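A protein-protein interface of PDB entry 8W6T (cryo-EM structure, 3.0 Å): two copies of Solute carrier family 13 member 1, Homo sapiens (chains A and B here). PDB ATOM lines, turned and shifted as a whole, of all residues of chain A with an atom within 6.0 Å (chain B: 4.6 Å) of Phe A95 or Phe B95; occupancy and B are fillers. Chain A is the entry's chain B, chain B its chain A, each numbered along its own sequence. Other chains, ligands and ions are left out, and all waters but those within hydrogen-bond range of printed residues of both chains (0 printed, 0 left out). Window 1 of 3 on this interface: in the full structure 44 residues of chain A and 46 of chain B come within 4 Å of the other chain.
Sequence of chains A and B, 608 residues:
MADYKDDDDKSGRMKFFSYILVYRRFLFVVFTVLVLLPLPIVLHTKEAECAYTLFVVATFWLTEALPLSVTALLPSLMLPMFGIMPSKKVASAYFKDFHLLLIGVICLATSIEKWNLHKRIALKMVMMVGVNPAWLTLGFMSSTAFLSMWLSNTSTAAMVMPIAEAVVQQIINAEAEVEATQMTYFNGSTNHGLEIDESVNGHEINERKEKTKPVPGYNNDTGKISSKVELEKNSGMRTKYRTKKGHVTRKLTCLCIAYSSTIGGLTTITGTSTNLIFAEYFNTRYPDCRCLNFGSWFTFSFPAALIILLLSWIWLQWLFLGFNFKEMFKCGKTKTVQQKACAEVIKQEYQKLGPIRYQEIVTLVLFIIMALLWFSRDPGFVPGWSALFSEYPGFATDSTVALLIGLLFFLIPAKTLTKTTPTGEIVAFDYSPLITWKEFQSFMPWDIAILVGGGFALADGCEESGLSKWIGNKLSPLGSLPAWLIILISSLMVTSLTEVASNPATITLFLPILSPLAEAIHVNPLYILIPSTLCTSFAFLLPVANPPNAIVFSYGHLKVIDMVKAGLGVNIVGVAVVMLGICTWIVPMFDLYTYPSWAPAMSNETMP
O of Phe B95 lies close to O of Ala A91 (3.1 Å). The backbone carbonyl oxygen (O) of Ala B91 sits close to the backbone carbonyl oxygen (O) of Phe A95.
Among the printed residues, merely in contact across the chains: Ser A92 with Ser B92 (3.5 Å), Ala A91 with Lys B96 (3.6 Å), Phe A95 with Tyr B94 (3.6 Å), Tyr A94 with Phe B95 (3.6 Å), Phe A95 with Phe B95 (3.7 Å), Lys A96 with Ala B91 (3.7 Å), Ser A92 with Phe B95 (3.7 Å), Phe A95 with Ser B92 (3.9 Å), Leu A100 with Ala B91 (3.9 Å) and Ala A91 with Leu B100 (3.97 Å).
Phe A95 touches four residues of chain B. Phe B95 touches four residues of chain A. Of the printed residues of chain A, Tyr B94 touches Phe A95 (3.6 Å). Of the printed residues of chain B, Lys A96 touches Ala B91 (3.7 Å). Of the printed residues of chain A, Ser B92 touches Ser A92 (3.5 Å) and Phe A95 (3.9 Å). Asp A97 touches none of the printed residues of chain B. His A99 touches none of the printed residues of chain B. The nearest residue of chain A that does not touch Phe B95 is Ile A450 (4.8 Å). The nearest printed residue of chain B that does not touch Ser A92 is Lys B96 (5.5 Å).
Printed residues of chain A that touch a printed residue of chain B: Ala A91, Ser A92, Tyr A94, Phe A95, Lys A96 and Leu A100. Along chain A the printed residues that touch a printed residue of chain B span positions 91 to 100. Of the 9 printed residues of chain B, 6 touch a printed residue of chain A. Hydrophobic or aromatic side chains of chain B that line the printed part of chain A: Ala B91, Tyr B94, Phe B95 and Leu B100. Among the printed residues, 12 pairs touch across the chains. Among the printed residues, no Asp or Glu carboxylate lies within 4 Å of a Lys or Arg side-chain nitrogen of the other chain.
Ala A91 touches Lys B96, and with the chains exchanged Lys A96 touches Ala B91. Ser B92 touches its own counterpart, Ser A92. Ser A92 touches Phe B95, and with the chains exchanged Phe A95 touches Ser B92. Tyr A94 touches Phe B95, and with the chains exchanged Phe A95 touches Tyr B94.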
ATOM      1  N   LYS A  88     -24.974  14.063  -7.757  1.00  0.00           N
ATOM      2  CA  LYS A  88     -26.317  13.726  -8.207  1.00  0.00           C
ATOM      3  C   LYS A  88     -26.797  14.641  -9.324  1.00  0.00           C
ATOM      4  O   LYS A  88     -27.791  14.324  -9.985  1.00  0.00           O
ATOM      5  CB  LYS A  88     -27.297  13.768  -7.034  1.00  0.00           C
ATOM      6  CG  LYS A  88     -27.411  15.120  -6.362  1.00  0.00           C
ATOM      7  CD  LYS A  88     -28.436  15.080  -5.242  1.00  0.00           C
ATOM      8  CE  LYS A  88     -27.978  14.170  -4.114  1.00  0.00           C
ATOM      9  NZ  LYS A  88     -28.856  14.279  -2.916  1.00  0.00           N
ATOM     10  N   ALA A  91     -25.077  12.896 -12.558  1.00  0.00           N
ATOM     11  CA  ALA A  91     -25.679  11.612 -12.898  1.00  0.00           C
ATOM     12  C   ALA A  91     -27.006  11.763 -13.630  1.00  0.00           C
ATOM     13  O   ALA A  91     -27.402  10.859 -14.373  1.00  0.00           O
ATOM     14  CB  ALA A  91     -25.872  10.777 -11.634  1.00  0.00           C
ATOM     15  N   SER A  92     -27.701  12.884 -13.445  1.00  0.00           N
ATOM     16  CA  SER A  92     -28.941  13.130 -14.168  1.00  0.00           C
ATOM     17  C   SER A  92     -28.721  13.404 -15.649  1.00  0.00           C
ATOM     18  O   SER A  92     -29.638  13.176 -16.445  1.00  0.00           O
ATOM     19  CB  SER A  92     -29.688  14.308 -13.542  1.00  0.00           C
ATOM     20  OG  SER A  92     -28.974  15.514 -13.732  1.00  0.00           O
ATOM     21  N   ALA A  93     -27.539  13.874 -16.037  1.00  0.00           N
ATOM     22  CA  ALA A  93     -27.228  14.184 -17.425  1.00  0.00           C
ATOM     23  C   ALA A  93     -26.821  12.958 -18.229  1.00  0.00           C
ATOM     24  O   ALA A  93     -26.640  13.062 -19.445  1.00  0.00           O
ATOM     25  CB  ALA A  93     -26.120  15.236 -17.492  1.00  0.00           C
ATOM     26  N   TYR A  94     -26.689  11.800 -17.588  1.00  0.00           N
ATOM     27  CA  TYR A  94     -26.257  10.584 -18.261  1.00  0.00           C
ATOM     28  C   TYR A  94     -27.405   9.794 -18.870  1.00  0.00           C
ATOM     29  O   TYR A  94     -27.177   8.686 -19.364  1.00  0.00           O
ATOM     30  CB  TYR A  94     -25.485   9.689 -17.288  1.00  0.00           C
ATOM     31  CG  TYR A  94     -24.006   9.970 -17.240  1.00  0.00           C
ATOM     32  CD1 TYR A  94     -23.497  10.959 -16.412  1.00  0.00           C
ATOM     33  CD2 TYR A  94     -23.118   9.247 -18.026  1.00  0.00           C
ATOM     34  CE1 TYR A  94     -22.145  11.220 -16.367  1.00  0.00           C
ATOM     35  CE2 TYR A  94     -21.764   9.501 -17.987  1.00  0.00           C
ATOM     36  CZ  TYR A  94     -21.285  10.491 -17.155  1.00  0.00           C
ATOM     37  OH  TYR A  94     -19.940  10.751 -17.108  1.00  0.00           O
ATOM     38  N   PHE A  95     -28.629  10.321 -18.838  1.00  0.00           N
ATOM     39  CA  PHE A  95     -29.761   9.639 -19.462  1.00  0.00           C
ATOM     40  C   PHE A  95     -30.747  10.731 -19.869  1.00  0.00           C
ATOM     41  O   PHE A  95     -31.551  11.182 -19.049  1.00  0.00           O
ATOM     42  CB  PHE A  95     -30.402   8.643 -18.507  1.00  0.00           C
ATOM     43  CG  PHE A  95     -31.220   7.582 -19.180  1.00  0.00           C
ATOM     44  CD1 PHE A  95     -30.631   6.404 -19.613  1.00  0.00           C
ATOM     45  CD2 PHE A  95     -32.576   7.769 -19.416  1.00  0.00           C
ATOM     46  CE1 PHE A  95     -31.375   5.420 -20.231  1.00  0.00           C
ATOM     47  CE2 PHE A  95     -33.327   6.794 -20.040  1.00  0.00           C
ATOM     48  CZ  PHE A  95     -32.727   5.617 -20.448  1.00  0.00           C
ATOM     49  N   LYS A  96     -30.672  11.152 -21.122  1.00  0.00           N
ATOM     50  CA  LYS A  96     -31.518  12.196 -21.666  1.00  0.00           C
ATOM     51  C   LYS A  96     -32.646  11.571 -22.483  1.00  0.00           C
ATOM     52  O   LYS A  96     -32.864  10.357 -22.464  1.00  0.00           O
ATOM     53  CB  LYS A  96     -30.684  13.164 -22.505  1.00  0.00           C
ATOM     54  CG  LYS A  96     -29.589  13.872 -21.732  1.00  0.00           C
ATOM     55  CD  LYS A  96     -30.096  15.162 -21.118  1.00  0.00           C
ATOM     56  CE  LYS A  96     -28.960  15.966 -20.518  1.00  0.00           C
ATOM     57  NZ  LYS A  96     -29.446  17.194 -19.830  1.00  0.00           N
ATOM     58  N   ASP A  97     -33.374  12.410 -23.213  1.00  0.00           N
ATOM     59  CA  ASP A  97     -34.489  11.952 -24.029  1.00  0.00           C
ATOM     60  C   ASP A  97     -34.031  11.244 -25.303  1.00  0.00           C
ATOM     61  O   ASP A  97     -34.860  10.653 -26.000  1.00  0.00           O
ATOM     62  CB  ASP A  97     -35.376  13.151 -24.374  1.00  0.00           C
ATOM     63  CG  ASP A  97     -36.807  12.760 -24.661  1.00  0.00           C
ATOM     64  OD1 ASP A  97     -37.139  11.569 -24.514  1.00  0.00           O
ATOM     65  OD2 ASP A  97     -37.603  13.645 -25.034  1.00  0.00           O
ATOM     66  N   HIS A  99     -32.047   8.663 -25.189  1.00  0.00           N
ATOM     67  CA  HIS A  99     -31.901   7.263 -24.816  1.00  0.00           C
ATOM     68  C   HIS A  99     -33.198   6.474 -24.935  1.00  0.00           C
ATOM     69  O   HIS A  99     -33.151   5.282 -25.251  1.00  0.00           O
ATOM     70  CB  HIS A  99     -31.358   7.169 -23.391  1.00  0.00           C
ATOM     71  CG  HIS A  99     -29.990   7.755 -23.226  1.00  0.00           C
ATOM     72  ND1 HIS A  99     -28.867   6.981 -23.042  1.00  0.00           N
ATOM     73  CD2 HIS A  99     -29.563   9.039 -23.233  1.00  0.00           C
ATOM     74  CE1 HIS A  99     -27.808   7.763 -22.933  1.00  0.00           C
ATOM     75  NE2 HIS A  99     -28.203   9.016 -23.046  1.00  0.00           N
ATOM     76  N   LEU A 100     -34.352   7.113 -24.725  1.00  0.00           N
ATOM     77  CA  LEU A 100     -35.626   6.429 -24.929  1.00  0.00           C
ATOM     78  C   LEU A 100     -35.872   6.124 -26.402  1.00  0.00           C
ATOM     79  O   LEU A 100     -36.335   5.026 -26.739  1.00  0.00           O
ATOM     80  CB  LEU A 100     -36.766   7.272 -24.364  1.00  0.00           C
ATOM     81  CG  LEU A 100     -36.645   7.722 -22.909  1.00  0.00           C
ATOM     82  CD1 LEU A 100     -37.774   8.667 -22.552  1.00  0.00           C
ATOM     83  CD2 LEU A 100     -36.631   6.529 -21.970  1.00  0.00           C
ATOM     84  N   ILE A 103     -33.631   3.261 -27.287  1.00  0.00           N
ATOM     85  CA  ILE A 103     -34.230   1.986 -26.903  1.00  0.00           C
ATOM     86  C   ILE A 103     -35.306   1.583 -27.906  1.00  0.00           C
ATOM     87  O   ILE A 103     -35.356   0.430 -28.359  1.00  0.00           O
ATOM     88  CB  ILE A 103     -34.787   2.074 -25.468  1.00  0.00           C
ATOM     89  CG1 ILE A 103     -33.644   2.124 -24.455  1.00  0.00           C
ATOM     90  CG2 ILE A 103     -35.696   0.894 -25.152  1.00  0.00           C
ATOM     91  CD1 ILE A 103     -34.101   2.299 -23.026  1.00  0.00           C
ATOM     92  N   ILE A 450     -23.417   5.464 -22.731  1.00  0.00           N
ATOM     93  CA  ILE A 450     -22.493   6.019 -21.747  1.00  0.00           C
ATOM     94  C   ILE A 450     -21.662   7.145 -22.354  1.00  0.00           C
ATOM     95  O   ILE A 450     -21.402   8.158 -21.698  1.00  0.00           O
ATOM     96  CB  ILE A 450     -21.611   4.895 -21.168  1.00  0.00           C
ATOM     97  CG1 ILE A 450     -22.480   3.787 -20.568  1.00  0.00           C
ATOM     98  CG2 ILE A 450     -20.656   5.423 -20.107  1.00  0.00           C
ATOM     99  CD1 ILE A 450     -23.284   4.210 -19.361  1.00  0.00           C
ATOM    100  N   GLY A 453     -23.986  10.187 -22.781  1.00  0.00           N
ATOM    101  CA  GLY A 453     -24.226  10.734 -21.458  1.00  0.00           C
ATOM    102  C   GLY A 453     -23.035  11.471 -20.880  1.00  0.00           C
ATOM    103  O   GLY A 453     -23.199  12.522 -20.255  1.00  0.00           O
ATOM    104  N   ALA B  91     -37.275  11.214 -18.277  1.00  0.00           N
ATOM    105  CA  ALA B  91     -36.046  10.559 -18.702  1.00  0.00           C
ATOM    106  C   ALA B  91     -34.877  10.854 -17.774  1.00  0.00           C
ATOM    107  O   ALA B  91     -33.942  10.054 -17.704  1.00  0.00           O
ATOM    108  CB  ALA B  91     -35.686  10.979 -20.129  1.00  0.00           C
ATOM    109  N   SER B  92     -34.920  11.964 -17.037  1.00  0.00           N
ATOM    110  CA  SER B  92     -33.869  12.338 -16.102  1.00  0.00           C
ATOM    111  C   SER B  92     -34.023  11.668 -14.740  1.00  0.00           C
ATOM    112  O   SER B  92     -33.336  12.052 -13.789  1.00  0.00           O
ATOM    113  CB  SER B  92     -33.836  13.857 -15.931  1.00  0.00           C
ATOM    114  OG  SER B  92     -32.859  14.235 -14.979  1.00  0.00           O
ATOM    115  N   ALA B  93     -34.912  10.683 -14.628  1.00  0.00           N
ATOM    116  CA  ALA B  93     -35.067   9.901 -13.415  1.00  0.00           C
ATOM    117  C   ALA B  93     -34.552   8.478 -13.563  1.00  0.00           C
ATOM    118  O   ALA B  93     -34.526   7.742 -12.571  1.00  0.00           O
ATOM    119  CB  ALA B  93     -36.539   9.872 -12.987  1.00  0.00           C
ATOM    120  N   TYR B  94     -34.140   8.071 -14.762  1.00  0.00           N
ATOM    121  CA  TYR B  94     -33.636   6.726 -15.003  1.00  0.00           C
ATOM    122  C   TYR B  94     -32.143   6.591 -14.733  1.00  0.00           C
ATOM    123  O   TYR B  94     -31.567   5.546 -15.050  1.00  0.00           O
ATOM    124  CB  TYR B  94     -33.925   6.302 -16.446  1.00  0.00           C
ATOM    125  CG  TYR B  94     -35.294   5.695 -16.659  1.00  0.00           C
ATOM    126  CD1 TYR B  94     -36.413   6.503 -16.812  1.00  0.00           C
ATOM    127  CD2 TYR B  94     -35.467   4.318 -16.713  1.00  0.00           C
ATOM    128  CE1 TYR B  94     -37.667   5.961 -17.005  1.00  0.00           C
ATOM    129  CE2 TYR B  94     -36.721   3.765 -16.907  1.00  0.00           C
ATOM    130  CZ  TYR B  94     -37.816   4.594 -17.052  1.00  0.00           C
ATOM    131  OH  TYR B  94     -39.067   4.059 -17.244  1.00  0.00           O
ATOM    132  N   PHE B  95     -31.504   7.617 -14.171  1.00  0.00           N
ATOM    133  CA  PHE B  95     -30.071   7.569 -13.876  1.00  0.00           C
ATOM    134  C   PHE B  95     -29.824   8.518 -12.708  1.00  0.00           C
ATOM    135  O   PHE B  95     -29.881   9.738 -12.875  1.00  0.00           O
ATOM    136  CB  PHE B  95     -29.242   7.953 -15.094  1.00  0.00           C
ATOM    137  CG  PHE B  95     -27.931   7.226 -15.200  1.00  0.00           C
ATOM    138  CD1 PHE B  95     -27.826   6.071 -15.957  1.00  0.00           C
ATOM    139  CD2 PHE B  95     -26.802   7.704 -14.554  1.00  0.00           C
ATOM    140  CE1 PHE B  95     -26.620   5.401 -16.063  1.00  0.00           C
ATOM    141  CE2 PHE B  95     -25.593   7.039 -14.655  1.00  0.00           C
ATOM    142  CZ  PHE B  95     -25.502   5.887 -15.410  1.00  0.00           C
ATOM    143  N   LYS B  96     -29.575   7.953 -11.537  1.00  0.00           N
ATOM    144  CA  LYS B  96     -29.288   8.695 -10.323  1.00  0.00           C
ATOM    145  C   LYS B  96     -27.901   8.310  -9.817  1.00  0.00           C
ATOM    146  O   LYS B  96     -27.123   7.649 -10.513  1.00  0.00           O
ATOM    147  CB  LYS B  96     -30.378   8.444  -9.277  1.00  0.00           C
ATOM    148  CG  LYS B  96     -31.786   8.675  -9.801  1.00  0.00           C
ATOM    149  CD  LYS B  96     -32.645   9.466  -8.836  1.00  0.00           C
ATOM    150  CE  LYS B  96     -33.949   9.877  -9.498  1.00  0.00           C
ATOM    151  NZ  LYS B  96     -34.844  10.622  -8.574  1.00  0.00           N
ATOM    152  N   HIS B  99     -26.562   4.637  -9.839  1.00  0.00           N
ATOM    153  CA  HIS B  99     -26.053   4.026 -11.058  1.00  0.00           C
ATOM    154  C   HIS B  99     -24.558   4.235 -11.248  1.00  0.00           C
ATOM    155  O   HIS B  99     -23.895   3.355 -11.805  1.00  0.00           O
ATOM    156  CB  HIS B  99     -26.820   4.567 -12.260  1.00  0.00           C
ATOM    157  CG  HIS B  99     -28.280   4.244 -12.229  1.00  0.00           C
ATOM    158  ND1 HIS B  99     -28.833   3.230 -12.979  1.00  0.00           N
ATOM    159  CD2 HIS B  99     -29.297   4.785 -11.520  1.00  0.00           C
ATOM    160  CE1 HIS B  99     -30.129   3.167 -12.737  1.00  0.00           C
ATOM    161  NE2 HIS B  99     -30.437   4.102 -11.857  1.00  0.00           N
ATOM    162  N   LEU B 100     -24.008   5.356 -10.777  1.00  0.00           N
ATOM    163  CA  LEU B 100     -22.560   5.537 -10.806  1.00  0.00           C
ATOM    164  C   LEU B 100     -21.864   4.578  -9.848  1.00  0.00           C
ATOM    165  O   LEU B 100     -20.806   4.027 -10.175  1.00  0.00           O
ATOM    166  CB  LEU B 100     -22.203   6.982 -10.461  1.00  0.00           C
ATOM    167  CG  LEU B 100     -22.763   8.076 -11.366  1.00  0.00           C
ATOM    168  CD1 LEU B 100     -22.206   9.425 -10.951  1.00  0.00           C
ATOM    169  CD2 LEU B 100     -22.448   7.785 -12.824  1.00  0.00           C
ATOM    170  N   ILE B 103     -22.000   1.181 -11.533  1.00  0.00           N
ATOM    171  CA  ILE B 103     -20.988   1.082 -12.581  1.00  0.00           C
ATOM    172  C   ILE B 103     -19.607   0.874 -11.965  1.00  0.00           C
ATOM    173  O   ILE B 103     -18.830   0.024 -12.417  1.00  0.00           O
ATOM    174  CB  ILE B 103     -21.039   2.330 -13.486  1.00  0.00           C
ATOM    175  CG1 ILE B 103     -22.202   2.222 -14.472  1.00  0.00           C
ATOM    176  CG2 ILE B 103     -19.738   2.536 -14.252  1.00  0.00           C
ATOM    177  CD1 ILE B 103     -22.372   3.437 -15.349  1.00  0.00           C
